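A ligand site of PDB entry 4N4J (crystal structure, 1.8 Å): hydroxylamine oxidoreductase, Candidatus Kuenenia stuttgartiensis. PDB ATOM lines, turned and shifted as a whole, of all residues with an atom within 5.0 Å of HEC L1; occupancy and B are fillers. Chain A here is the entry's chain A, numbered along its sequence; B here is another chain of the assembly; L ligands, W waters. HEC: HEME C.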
ATOM      1  N   TRP A  58      33.043  14.007 -17.215  1.00  0.00           N
ATOM      2  CA  TRP A  58      31.926  14.873 -16.822  1.00  0.00           C
ATOM      3  C   TRP A  58      32.140  15.543 -15.468  1.00  0.00           C
ATOM      4  O   TRP A  58      31.539  16.580 -15.188  1.00  0.00           O
ATOM      5  CB  TRP A  58      30.601  14.097 -16.800  1.00  0.00           C
ATOM      6  CG  TRP A  58      30.349  13.376 -18.078  1.00  0.00           C
ATOM      7  CD1 TRP A  58      30.673  12.090 -18.362  1.00  0.00           C
ATOM      8  CD2 TRP A  58      29.761  13.915 -19.256  1.00  0.00           C
ATOM      9  NE1 TRP A  58      30.325  11.783 -19.642  1.00  0.00           N
ATOM     10  CE2 TRP A  58      29.763  12.888 -20.223  1.00  0.00           C
ATOM     11  CE3 TRP A  58      29.234  15.163 -19.594  1.00  0.00           C
ATOM     12  CZ2 TRP A  58      29.247  13.073 -21.500  1.00  0.00           C
ATOM     13  CZ3 TRP A  58      28.731  15.344 -20.870  1.00  0.00           C
ATOM     14  CH2 TRP A  58      28.735  14.308 -21.808  1.00  0.00           C
ATOM     15  N   TRP A  65      37.967  16.498 -19.844  1.00  0.00           N
ATOM     16  CA  TRP A  65      36.959  16.763 -20.862  1.00  0.00           C
ATOM     17  C   TRP A  65      37.600  16.936 -22.229  1.00  0.00           C
ATOM     18  O   TRP A  65      38.593  17.655 -22.377  1.00  0.00           O
ATOM     19  CB  TRP A  65      36.134  18.003 -20.531  1.00  0.00           C
ATOM     20  CG  TRP A  65      35.093  18.275 -21.558  1.00  0.00           C
ATOM     21  CD1 TRP A  65      35.113  19.250 -22.498  1.00  0.00           C
ATOM     22  CD2 TRP A  65      33.887  17.524 -21.763  1.00  0.00           C
ATOM     23  NE1 TRP A  65      33.978  19.180 -23.270  1.00  0.00           N
ATOM     24  CE2 TRP A  65      33.211  18.122 -22.847  1.00  0.00           C
ATOM     25  CE3 TRP A  65      33.313  16.417 -21.128  1.00  0.00           C
ATOM     26  CZ2 TRP A  65      31.990  17.651 -23.317  1.00  0.00           C
ATOM     27  CZ3 TRP A  65      32.099  15.940 -21.603  1.00  0.00           C
ATOM     28  CH2 TRP A  65      31.450  16.552 -22.688  1.00  0.00           C
ATOM     29  N   GLY A  68      33.602  15.192 -27.901  1.00  0.00           N
ATOM     30  CA  GLY A  68      33.120  13.874 -28.319  1.00  0.00           C
ATOM     31  C   GLY A  68      31.791  13.964 -29.034  1.00  0.00           C
ATOM     32  O   GLY A  68      31.010  13.016 -29.035  1.00  0.00           O
ATOM     33  N   SER A  69      31.537  15.111 -29.663  1.00  0.00           N
ATOM     34  CA  SER A  69      30.295  15.345 -30.363  1.00  0.00           C
ATOM     35  C   SER A  69      30.479  15.059 -31.846  1.00  0.00           C
ATOM     36  O   SER A  69      31.581  15.185 -32.379  1.00  0.00           O
ATOM     37  CB  SER A  69      29.847  16.799 -30.182  1.00  0.00           C
ATOM     38  OG  SER A  69      28.635  17.038 -30.855  1.00  0.00           O
ATOM     39  N   GLN A  70      29.394  14.656 -32.496  1.00  0.00           N
ATOM     40  CA  GLN A  70      29.371  14.411 -33.932  1.00  0.00           C
ATOM     41  C   GLN A  70      28.740  15.572 -34.696  1.00  0.00           C
ATOM     42  O   GLN A  70      28.775  15.603 -35.936  1.00  0.00           O
ATOM     43  CB  GLN A  70      28.602  13.116 -34.232  1.00  0.00           C
ATOM     44  CG  GLN A  70      29.262  11.863 -33.685  1.00  0.00           C
ATOM     45  CD  GLN A  70      29.263  11.818 -32.161  1.00  0.00           C
ATOM     46  OE1 GLN A  70      30.318  11.655 -31.542  1.00  0.00           O
ATOM     47  NE2 GLN A  70      28.095  11.985 -31.552  1.00  0.00           N
ATOM     48  N   THR A  71      28.158  16.520 -33.973  1.00  0.00           N
ATOM     49  CA  THR A  71      27.480  17.651 -34.583  1.00  0.00           C
ATOM     50  C   THR A  71      28.479  18.784 -34.779  1.00  0.00           C
ATOM     51  O   THR A  71      29.201  19.157 -33.853  1.00  0.00           O
ATOM     52  CB  THR A  71      26.298  18.121 -33.709  1.00  0.00           C
ATOM     53  OG1 THR A  71      25.339  17.057 -33.623  1.00  0.00           O
ATOM     54  CG2 THR A  71      25.626  19.352 -34.285  1.00  0.00           C
ATOM     55  N   PHE A  75      26.984  27.985 -33.528  1.00  0.00           N
ATOM     56  CA  PHE A  75      25.571  28.334 -33.407  1.00  0.00           C
ATOM     57  C   PHE A  75      25.330  29.445 -32.398  1.00  0.00           C
ATOM     58  O   PHE A  75      26.092  29.615 -31.447  1.00  0.00           O
ATOM     59  CB  PHE A  75      24.768  27.113 -32.978  1.00  0.00           C
ATOM     60  CG  PHE A  75      24.907  25.941 -33.901  1.00  0.00           C
ATOM     61  CD1 PHE A  75      24.290  25.953 -35.147  1.00  0.00           C
ATOM     62  CD2 PHE A  75      25.643  24.829 -33.527  1.00  0.00           C
ATOM     63  CE1 PHE A  75      24.420  24.869 -36.003  1.00  0.00           C
ATOM     64  CE2 PHE A  75      25.773  23.744 -34.384  1.00  0.00           C
ATOM     65  CZ  PHE A  75      25.153  23.770 -35.628  1.00  0.00           C
ATOM     66  N   LYS A  76      24.244  30.191 -32.624  1.00  0.00           N
ATOM     67  CA  LYS A  76      23.761  31.175 -31.660  1.00  0.00           C
ATOM     68  C   LYS A  76      22.897  30.456 -30.634  1.00  0.00           C
ATOM     69  O   LYS A  76      22.325  29.398 -30.919  1.00  0.00           O
ATOM     70  CB  LYS A  76      22.924  32.237 -32.370  1.00  0.00           C
ATOM     71  CG  LYS A  76      23.658  33.030 -33.434  1.00  0.00           C
ATOM     72  CD  LYS A  76      22.689  33.900 -34.234  1.00  0.00           C
ATOM     73  CE  LYS A  76      23.423  34.783 -35.242  1.00  0.00           C
ATOM     74  NZ  LYS A  76      22.486  35.713 -35.955  1.00  0.00           N
ATOM     75  N   GLU A  79      19.657  28.922 -31.720  1.00  0.00           N
ATOM     76  CA  GLU A  79      19.837  27.722 -32.536  1.00  0.00           C
ATOM     77  C   GLU A  79      20.084  26.482 -31.666  1.00  0.00           C
ATOM     78  O   GLU A  79      19.559  25.406 -31.952  1.00  0.00           O
ATOM     79  CB  GLU A  79      20.985  27.924 -33.534  1.00  0.00           C
ATOM     80  CG  GLU A  79      20.633  28.950 -34.605  1.00  0.00           C
ATOM     81  CD  GLU A  79      21.804  29.338 -35.486  1.00  0.00           C
ATOM     82  OE1 GLU A  79      21.567  29.613 -36.676  1.00  0.00           O
ATOM     83  OE2 GLU A  79      22.954  29.390 -35.001  1.00  0.00           O
ATOM     84  N   CYS A  80      20.876  26.643 -30.601  1.00  0.00           N
ATOM     85  CA  CYS A  80      21.040  25.585 -29.606  1.00  0.00           C
ATOM     86  C   CYS A  80      19.668  25.107 -29.153  1.00  0.00           C
ATOM     87  O   CYS A  80      19.400  23.909 -29.120  1.00  0.00           O
ATOM     88  CB  CYS A  80      21.799  26.059 -28.359  1.00  0.00           C
ATOM     89  SG  CYS A  80      23.319  26.965 -28.604  1.00  0.00           S
ATOM     90  N   CYS A  83      17.283  23.226 -31.939  1.00  0.00           N
ATOM     91  CA  CYS A  83      17.655  21.856 -32.215  1.00  0.00           C
ATOM     92  C   CYS A  83      17.492  20.971 -30.985  1.00  0.00           C
ATOM     93  O   CYS A  83      16.976  19.861 -31.087  1.00  0.00           O
ATOM     94  CB  CYS A  83      19.088  21.773 -32.691  1.00  0.00           C
ATOM     95  SG  CYS A  83      19.496  20.158 -33.352  1.00  0.00           S
ATOM     96  N   HIS A  84      17.948  21.445 -29.831  1.00  0.00           N
ATOM     97  CA  HIS A  84      17.855  20.664 -28.605  1.00  0.00           C
ATOM     98  C   HIS A  84      16.436  20.491 -28.084  1.00  0.00           C
ATOM     99  O   HIS A  84      16.184  19.615 -27.270  1.00  0.00           O
ATOM    100  CB  HIS A  84      18.791  21.201 -27.521  1.00  0.00           C
ATOM    101  CG  HIS A  84      20.192  20.707 -27.677  1.00  0.00           C
ATOM    102  ND1 HIS A  84      20.627  19.527 -27.098  1.00  0.00           N
ATOM    103  CD2 HIS A  84      21.226  21.181 -28.403  1.00  0.00           C
ATOM    104  CE1 HIS A  84      21.883  19.325 -27.430  1.00  0.00           C
ATOM    105  NE2 HIS A  84      22.270  20.304 -28.227  1.00  0.00           N
ATOM    106  N   GLN A  87      16.298  17.314 -29.807  1.00  0.00           N
ATOM    107  CA  GLN A  87      17.334  16.337 -29.490  1.00  0.00           C
ATOM    108  C   GLN A  87      17.477  15.994 -28.004  1.00  0.00           C
ATOM    109  O   GLN A  87      17.802  14.859 -27.680  1.00  0.00           O
ATOM    110  CB  GLN A  87      18.679  16.787 -30.055  1.00  0.00           C
ATOM    111  CG  GLN A  87      18.743  16.701 -31.579  1.00  0.00           C
ATOM    112  CD  GLN A  87      18.516  15.291 -32.084  1.00  0.00           C
ATOM    113  OE1 GLN A  87      19.001  14.327 -31.493  1.00  0.00           O
ATOM    114  NE2 GLN A  87      17.763  15.155 -33.165  1.00  0.00           N
ATOM    115  N   CYS A 124      22.392  28.290 -23.721  1.00  0.00           N
ATOM    116  CA  CYS A 124      23.235  27.102 -23.833  1.00  0.00           C
ATOM    117  C   CYS A 124      24.659  27.484 -24.207  1.00  0.00           C
ATOM    118  O   CYS A 124      25.616  26.986 -23.631  1.00  0.00           O
ATOM    119  CB  CYS A 124      22.700  26.113 -24.890  1.00  0.00           C
ATOM    120  SG  CYS A 124      20.927  25.884 -24.949  1.00  0.00           S
ATOM    121  N   ALA A 125      24.800  28.375 -25.198  1.00  0.00           N
ATOM    122  CA  ALA A 125      26.112  28.755 -25.716  1.00  0.00           C
ATOM    123  C   ALA A 125      26.924  29.568 -24.713  1.00  0.00           C
ATOM    124  O   ALA A 125      28.153  29.531 -24.713  1.00  0.00           O
ATOM    125  CB  ALA A 125      25.977  29.511 -27.052  1.00  0.00           C
ATOM    126  N   HIS A 128      28.133  26.653 -22.464  1.00  0.00           N
ATOM    127  CA  HIS A 128      28.807  25.517 -23.119  1.00  0.00           C
ATOM    128  C   HIS A 128      29.691  25.882 -24.322  1.00  0.00           C
ATOM    129  O   HIS A 128      30.389  25.012 -24.846  1.00  0.00           O
ATOM    130  CB  HIS A 128      27.762  24.494 -23.544  1.00  0.00           C
ATOM    131  CG  HIS A 128      27.086  23.818 -22.401  1.00  0.00           C
ATOM    132  ND1 HIS A 128      27.732  22.920 -21.582  1.00  0.00           N
ATOM    133  CD2 HIS A 128      25.820  23.912 -21.925  1.00  0.00           C
ATOM    134  CE1 HIS A 128      26.897  22.479 -20.662  1.00  0.00           C
ATOM    135  NE2 HIS A 128      25.731  23.071 -20.851  1.00  0.00           N
ATOM    136  N   GLY A 129      29.649  27.131 -24.754  1.00  0.00           N
ATOM    137  CA  GLY A 129      30.376  27.568 -25.952  1.00  0.00           C
ATOM    138  C   GLY A 129      29.484  27.489 -27.173  1.00  0.00           C
ATOM    139  O   GLY A 129      28.443  26.841 -27.147  1.00  0.00           O
ATOM    140  N   ASN A 130      29.898  28.182 -28.238  1.00  0.00           N
ATOM    141  CA  ASN A 130      29.121  28.279 -29.478  1.00  0.00           C
ATOM    142  C   ASN A 130      29.469  27.218 -30.520  1.00  0.00           C
ATOM    143  O   ASN A 130      28.649  26.887 -31.367  1.00  0.00           O
ATOM    144  CB  ASN A 130      29.296  29.662 -30.112  1.00  0.00           C
ATOM    145  CG  ASN A 130      28.752  30.777 -29.254  1.00  0.00           C
ATOM    146  OD1 ASN A 130      29.444  31.285 -28.364  1.00  0.00           O
ATOM    147  ND2 ASN A 130      27.518  31.176 -29.514  1.00  0.00           N
ATOM    148  N   HIS A 132      30.128  23.560 -31.722  1.00  0.00           N
ATOM    149  CA  HIS A 132      29.649  22.258 -31.294  1.00  0.00           C
ATOM    150  C   HIS A 132      30.734  21.176 -31.269  1.00  0.00           C
ATOM    151  O   HIS A 132      30.525  20.091 -30.724  1.00  0.00           O
ATOM    152  CB  HIS A 132      28.455  21.800 -32.140  1.00  0.00           C
ATOM    153  CG  HIS A 132      27.459  21.009 -31.356  1.00  0.00           C
ATOM    154  ND1 HIS A 132      27.689  19.706 -30.964  1.00  0.00           N
ATOM    155  CD2 HIS A 132      26.247  21.333 -30.859  1.00  0.00           C
ATOM    156  CE1 HIS A 132      26.646  19.262 -30.277  1.00  0.00           C
ATOM    157  NE2 HIS A 132      25.762  20.231 -30.200  1.00  0.00           N
ATOM    158  N   LEU A 135      32.631  22.121 -27.432  1.00  0.00           N
ATOM    159  CA  LEU A 135      31.722  22.348 -26.320  1.00  0.00           C
ATOM    160  C   LEU A 135      32.461  22.228 -24.994  1.00  0.00           C
ATOM    161  O   LEU A 135      33.444  21.501 -24.868  1.00  0.00           O
ATOM    162  CB  LEU A 135      30.527  21.391 -26.371  1.00  0.00           C
ATOM    163  CG  LEU A 135      29.596  21.635 -27.550  1.00  0.00           C
ATOM    164  CD1 LEU A 135      28.657  20.458 -27.726  1.00  0.00           C
ATOM    165  CD2 LEU A 135      28.809  22.943 -27.400  1.00  0.00           C
ATOM    166  N   MET A 137      32.371  21.691 -20.765  1.00  0.00           N
ATOM    167  CA  MET A 137      31.662  21.040 -19.664  1.00  0.00           C
ATOM    168  C   MET A 137      32.108  21.743 -18.381  1.00  0.00           C
ATOM    169  O   MET A 137      33.222  21.509 -17.897  1.00  0.00           O
ATOM    170  CB  MET A 137      31.967  19.550 -19.634  1.00  0.00           C
ATOM    171  CG  MET A 137      30.902  18.699 -18.942  1.00  0.00           C
ATOM    172  SD  MET A 137      29.186  19.090 -19.383  1.00  0.00           S
ATOM    173  CE  MET A 137      29.170  18.975 -21.166  1.00  0.00           C
ATOM    174  N   GLN B 311      18.468  10.022 -23.791  1.00  0.00           N
ATOM    175  CA  GLN B 311      18.655  11.258 -24.557  1.00  0.00           C
ATOM    176  C   GLN B 311      17.409  12.153 -24.571  1.00  0.00           C
ATOM    177  O   GLN B 311      17.496  13.306 -24.961  1.00  0.00           O
ATOM    178  CB  GLN B 311      19.103  10.951 -25.990  1.00  0.00           C
ATOM    179  CG  GLN B 311      19.592  12.185 -26.734  1.00  0.00           C
ATOM    180  CD  GLN B 311      20.034  11.913 -28.153  1.00  0.00           C
ATOM    181  OE1 GLN B 311      20.465  10.810 -28.491  1.00  0.00           O
ATOM    182  NE2 GLN B 311      19.950  12.936 -29.007  1.00  0.00           N
ATOM    183  N   SER B 315      22.622  14.286 -22.873  1.00  0.00           N
ATOM    184  CA  SER B 315      23.548  13.936 -23.938  1.00  0.00           C
ATOM    185  C   SER B 315      23.587  12.418 -24.092  1.00  0.00           C
ATOM    186  O   SER B 315      23.643  11.706 -23.102  1.00  0.00           O
ATOM    187  CB  SER B 315      24.944  14.409 -23.591  1.00  0.00           C
ATOM    188  OG  SER B 315      25.902  13.739 -24.387  1.00  0.00           O
ATOM    189  N   PRO B 316      23.570  11.912 -25.344  1.00  0.00           N
ATOM    190  CA  PRO B 316      23.707  10.463 -25.525  1.00  0.00           C
ATOM    191  C   PRO B 316      25.089   9.953 -25.153  1.00  0.00           C
ATOM    192  O   PRO B 316      25.253   8.772 -24.844  1.00  0.00           O
ATOM    193  CB  PRO B 316      23.446  10.274 -27.015  1.00  0.00           C
ATOM    194  CG  PRO B 316      23.836  11.562 -27.637  1.00  0.00           C
ATOM    195  CD  PRO B 316      23.489  12.618 -26.625  1.00  0.00           C
ATOM    196  N   ARG B 317      26.091  10.827 -25.207  1.00  0.00           N
ATOM    197  CA  ARG B 317      27.438  10.487 -24.785  1.00  0.00           C
ATOM    198  C   ARG B 317      27.465  10.260 -23.272  1.00  0.00           C
ATOM    199  O   ARG B 317      28.070   9.312 -22.792  1.00  0.00           O
ATOM    200  CB  ARG B 317      28.403  11.602 -25.146  1.00  0.00           C
ATOM    201  CG  ARG B 317      29.861  11.308 -24.875  1.00  0.00           C
ATOM    202  CD  ARG B 317      30.659  12.577 -25.018  1.00  0.00           C
ATOM    203  NE  ARG B 317      32.096  12.385 -24.902  1.00  0.00           N
ATOM    204  CZ  ARG B 317      32.981  13.380 -24.900  1.00  0.00           C
ATOM    205  NH1 ARG B 317      32.585  14.642 -25.013  1.00  0.00           N
ATOM    206  NH2 ARG B 317      34.278  13.110 -24.799  1.00  0.00           N
ATOM    207  N   PHE B 318      26.803  11.145 -22.542  1.00  0.00           N
ATOM    208  CA  PHE B 318      26.676  11.002 -21.087  1.00  0.00           C
ATOM    209  C   PHE B 318      25.959   9.699 -20.731  1.00  0.00           C
ATOM    210  O   PHE B 318      26.433   8.924 -19.887  1.00  0.00           O
ATOM    211  CB  PHE B 318      25.916  12.196 -20.512  1.00  0.00           C
ATOM    212  CG  PHE B 318      25.690  12.101 -19.035  1.00  0.00           C
ATOM    213  CD1 PHE B 318      26.757  12.081 -18.164  1.00  0.00           C
ATOM    214  CD2 PHE B 318      24.404  12.019 -18.522  1.00  0.00           C
ATOM    215  CE1 PHE B 318      26.564  11.987 -16.794  1.00  0.00           C
ATOM    216  CE2 PHE B 318      24.200  11.916 -17.154  1.00  0.00           C
ATOM    217  CZ  PHE B 318      25.274  11.913 -16.293  1.00  0.00           C
HETATM  218 FE   HEC L   1      23.999  20.319 -29.227  1.00  0.00          FE
HETATM  219  CHA HEC L   1      25.054  17.339 -27.949  1.00  0.00           C
HETATM  220  CHB HEC L   1      25.080  21.927 -26.426  1.00  0.00           C
HETATM  221  CHC HEC L   1      23.563  23.327 -30.814  1.00  0.00           C
HETATM  222  CHD HEC L   1      22.313  18.739 -31.742  1.00  0.00           C
HETATM  223  NA  HEC L   1      24.877  19.742 -27.488  1.00  0.00           N
HETATM  224  C1A HEC L   1      25.295  18.463 -27.191  1.00  0.00           C
HETATM  225  C2A HEC L   1      26.019  18.513 -25.937  1.00  0.00           C
HETATM  226  C3A HEC L   1      26.038  19.776 -25.510  1.00  0.00           C
HETATM  227  C4A HEC L   1      25.308  20.572 -26.485  1.00  0.00           C
HETATM  228  CMA HEC L   1      26.689  20.324 -24.222  1.00  0.00           C
HETATM  229  CAA HEC L   1      26.676  17.280 -25.287  1.00  0.00           C
HETATM  230  CBA HEC L   1      28.018  17.091 -25.998  1.00  0.00           C
HETATM  231  CGA HEC L   1      28.717  15.827 -25.575  1.00  0.00           C
HETATM  232  O1A HEC L   1      28.047  14.815 -25.247  1.00  0.00           O
HETATM  233  O2A HEC L   1      29.967  15.837 -25.562  1.00  0.00           O
HETATM  234  NB  HEC L   1      24.233  22.262 -28.704  1.00  0.00           N
HETATM  235  C1B HEC L   1      24.774  22.710 -27.518  1.00  0.00           C
HETATM  236  C2B HEC L   1      24.962  24.136 -27.624  1.00  0.00           C
HETATM  237  C3B HEC L   1      24.546  24.523 -28.838  1.00  0.00           C
HETATM  238  C4B HEC L   1      24.069  23.351 -29.532  1.00  0.00           C
HETATM  239  CMB HEC L   1      25.553  25.056 -26.527  1.00  0.00           C
HETATM  240  CAB HEC L   1      24.572  25.951 -29.399  1.00  0.00           C
HETATM  241  CBB HEC L   1      25.732  26.611 -29.391  1.00  0.00           C
HETATM  242  NC  HEC L   1      23.119  20.917 -30.953  1.00  0.00           N
HETATM  243  C1C HEC L   1      23.038  22.218 -31.425  1.00  0.00           C
HETATM  244  C2C HEC L   1      22.308  22.202 -32.665  1.00  0.00           C
HETATM  245  C3C HEC L   1      21.955  20.925 -32.921  1.00  0.00           C
HETATM  246  C4C HEC L   1      22.461  20.111 -31.842  1.00  0.00           C
HETATM  247  CMC HEC L   1      21.995  23.454 -33.513  1.00  0.00           C
HETATM  248  CAC HEC L   1      21.130  20.372 -34.115  1.00  0.00           C
HETATM  249  CBC HEC L   1      21.051  21.054 -35.264  1.00  0.00           C
HETATM  250  ND  HEC L   1      23.719  18.366 -29.758  1.00  0.00           N
HETATM  251  C1D HEC L   1      22.967  17.939 -30.847  1.00  0.00           C
HETATM  252  C2D HEC L   1      22.982  16.495 -30.902  1.00  0.00           C
HETATM  253  C3D HEC L   1      23.841  16.065 -29.718  1.00  0.00           C
HETATM  254  C4D HEC L   1      24.255  17.283 -29.068  1.00  0.00           C
HETATM  255  CMD HEC L   1      22.285  15.588 -31.936  1.00  0.00           C
HETATM  256  CAD HEC L   1      24.178  14.628 -29.326  1.00  0.00           C
HETATM  257  CBD HEC L   1      25.019  13.990 -30.427  1.00  0.00           C
HETATM  258  CGD HEC L   1      26.218  14.838 -30.751  1.00  0.00           C
HETATM  259  O1D HEC L   1      26.440  15.074 -31.973  1.00  0.00           O
HETATM  260  O2D HEC L   1      26.957  15.267 -29.822  1.00  0.00           O
HETATM  261 FE   HEC L   2      24.030  22.646 -19.838  1.00  0.00          FE
HETATM  262  CHA HEC L   2      25.610  19.875 -18.573  1.00  0.00           C
HETATM  263  CHB HEC L   2      23.171  20.923 -22.617  1.00  0.00           C
HETATM  264  CHC HEC L   2      22.087  25.293 -20.825  1.00  0.00           C
HETATM  265  CHD HEC L   2      25.371  24.606 -17.381  1.00  0.00           C
HETATM  266  NA  HEC L   2      24.328  20.731 -20.465  1.00  0.00           N
HETATM  267  C1A HEC L   2      25.015  19.745 -19.802  1.00  0.00           C
HETATM  268  C2A HEC L   2      24.983  18.553 -20.633  1.00  0.00           C
HETATM  269  C3A HEC L   2      24.316  18.851 -21.760  1.00  0.00           C
HETATM  270  C4A HEC L   2      23.882  20.227 -21.668  1.00  0.00           C
HETATM  271  CMA HEC L   2      24.023  17.923 -22.960  1.00  0.00           C
HETATM  272  CAA HEC L   2      25.675  17.220 -20.277  1.00  0.00           C
HETATM  273  CBA HEC L   2      25.044  16.543 -19.064  1.00  0.00           C
HETATM  274  CGA HEC L   2      23.824  15.754 -19.480  1.00  0.00           C
HETATM  275  O1A HEC L   2      22.882  15.681 -18.657  1.00  0.00           O
HETATM  276  O2A HEC L   2      23.802  15.200 -20.603  1.00  0.00           O
HETATM  277  NB  HEC L   2      22.872  23.042 -21.418  1.00  0.00           N
HETATM  278  C1B HEC L   2      22.635  22.175 -22.469  1.00  0.00           C
HETATM  279  C2B HEC L   2      21.726  22.820 -23.379  1.00  0.00           C
HETATM  280  C3B HEC L   2      21.427  24.014 -22.873  1.00  0.00           C
HETATM  281  C4B HEC L   2      22.136  24.179 -21.637  1.00  0.00           C
HETATM  282  CMB HEC L   2      21.184  22.206 -24.695  1.00  0.00           C
HETATM  283  CAB HEC L   2      20.460  25.069 -23.418  1.00  0.00           C
HETATM  284  CBB HEC L   2      19.165  24.741 -23.519  1.00  0.00           C
HETATM  285  NC  HEC L   2      23.739  24.591 -19.196  1.00  0.00           N
HETATM  286  C1C HEC L   2      22.972  25.547 -19.814  1.00  0.00           C
HETATM  287  C2C HEC L   2      23.252  26.824 -19.210  1.00  0.00           C
HETATM  288  C3C HEC L   2      24.172  26.638 -18.260  1.00  0.00           C
HETATM  289  C4C HEC L   2      24.493  25.225 -18.231  1.00  0.00           C
HETATM  290  CMC HEC L   2      22.613  28.167 -19.622  1.00  0.00           C
HETATM  291  CAC HEC L   2      24.802  27.737 -17.378  1.00  0.00           C
HETATM  292  CBC HEC L   2      24.008  28.460 -16.572  1.00  0.00           C
HETATM  293  ND  HEC L   2      25.246  22.284 -18.224  1.00  0.00           N
HETATM  294  C1D HEC L   2      25.714  23.281 -17.374  1.00  0.00           C
HETATM  295  C2D HEC L   2      26.657  22.708 -16.440  1.00  0.00           C
HETATM  296  C3D HEC L   2      26.733  21.244 -16.800  1.00  0.00           C
HETATM  297  C4D HEC L   2      25.828  21.059 -17.918  1.00  0.00           C
HETATM  298  CMD HEC L   2      27.427  23.421 -15.318  1.00  0.00           C
HETATM  299  CAD HEC L   2      27.645  20.195 -16.127  1.00  0.00           C
HETATM  300  CBD HEC L   2      26.859  19.250 -15.244  1.00  0.00           C
HETATM  301  CGD HEC L   2      26.489  19.891 -13.934  1.00  0.00           C
HETATM  302  O1D HEC L   2      25.462  19.466 -13.354  1.00  0.00           O
HETATM  303  O2D HEC L   2      27.221  20.805 -13.457  1.00  0.00           O
HETATM  304  O   HOH W   1      31.817  17.149 -26.909  1.00  0.00           O
HETATM  305  O   HOH W   2      26.939  13.809 -27.617  1.00  0.00           O
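The side-chain amide oxygen (OE1) of Gln 70 sits close to the backbone carbonyl oxygen (O) of Gly 68 (2.9 Å).
OE1 of Gln 87 lies within hydrogen-bond range of NE2 of Gln 311 of chain B, 3.0 Å away.
OG of Ser 69 lies within hydrogen-bond range of N of Thr 71, at 3.2 Å.
The side-chain hydroxyl (OG) of Ser 315 of chain B lies within hydrogen-bond range of the backbone NH (N) of Arg 317 of chain B (3.0 Å).
The side-chain hydroxyl (OG) of Ser 315 of chain B sits at hydrogen-bond distance from the backbone NH (N) of Phe 318 of chain B.
The side-chain carboxylate of Glu 79 lies within hydrogen-bond range of the backbone NH of Lys 76 (2.8 Å).
NE1 of Trp 65 is in hydrogen-bond range of O of Leu 135, at 2.9 Å.
A ring nitrogen (ND1) of His 132 lies close to the backbone carbonyl oxygen of Thr 71 (3.3 Å).
Trp 58 touches HEC L1.
CH2 of Trp 65 touches O2A of HEC L1, at 3.3 Å.
Phe 75 touches HEC L1.
O of Glu 79 touches CMC of HEC L1 (3.5 Å).
Gln 87 touches HEC L1 (OE1 to CMD, 3.5 Å).
Cys 124 touches HEC L1.
Ala 125 touches HEC L1.
CB of His 128 touches CMB of HEC L1 (3.8 Å).
Gly 129 touches HEC L1 (O to CMB, 3.5 Å).
Asn 130 touches HEC L1 (O to CBB, 3.5 Å).
CD1 of Leu 135 touches C3A of HEC L1, at 3.5 Å.
Pro 316 of chain B touches HEC L1 (CD to CAD, 3.4 Å).
Hydrophobic or aromatic side chains that line HEC L1: Trp 58, Trp 65, Phe 75, His 84, Ala 125, His 128, His 132, Leu 135 and Pro 316 of chain B.
Within 4 Å of HEC L1: Trp 58, Trp 65, Ser 69, Gln 70, Thr 71, Phe 75, Glu 79, Cys 80, Cys 83, His 84, Gln 87, Cys 124, Ala 125, His 128, Gly 129, Asn 130, His 132, Leu 135, Ser 315 of chain B, Pro 316 of chain B and Arg 317 of chain B.
The nearest printed residue that does not touch HEC L1 is Met 137 (4.2 Å).
Water W2 bridges an oxygen (O2D) of HEC L1 (2.6 Å) and the side-chain hydroxyl (OG) of Ser 315 of chain B (3.4 Å).
The side-chain hydroxyl of Ser 69 sits at hydrogen-bond distance from an oxygen (O2D) of HEC L1 (2.6 Å).
The side-chain hydroxyl of Ser 315 of chain B is in hydrogen-bond range of an oxygen (O1A) of HEC L1, at 2.5 Å.
N of Gln 70 sits at hydrogen-bond distance from O1D of HEC L1.
The backbone NH of Ser 315 of chain B is in hydrogen-bond range of an oxygen (O2A) of HEC L2, 2.7 Å away.
A ring nitrogen (NE2) of His 132 is bound to an iron atom (FE) of HEC L1.
The side-chain sulfur (SG) of Cys 80 is covalently linked to a carbon (CAB) of HEC L1, at 1.8 Å.
The side-chain sulfur (SG) of Cys 83 is covalently linked to a carbon (CAC) of HEC L1 (1.8 Å).
N of Thr 71 sits at hydrogen-bond distance from O1D of HEC L1 (3.0 Å).
An iron atom (FE) of HEC L1 is bound by a ring nitrogen (NE2) of His 84.
The side-chain hydroxyl (OG1) of Thr 71 sits at hydrogen-bond distance from an oxygen (O1D) of HEC L1, at 2.8 Å.
NE2 of His 128 is bound to FE of HEC L2 (2.0 Å).
CAB of HEC L2 is bonded to SG of Cys 124, 1.8 Å away.
NH1 of Arg 317 of chain B is in salt-bridge range of O2A of HEC L1, at 2.9 Å.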
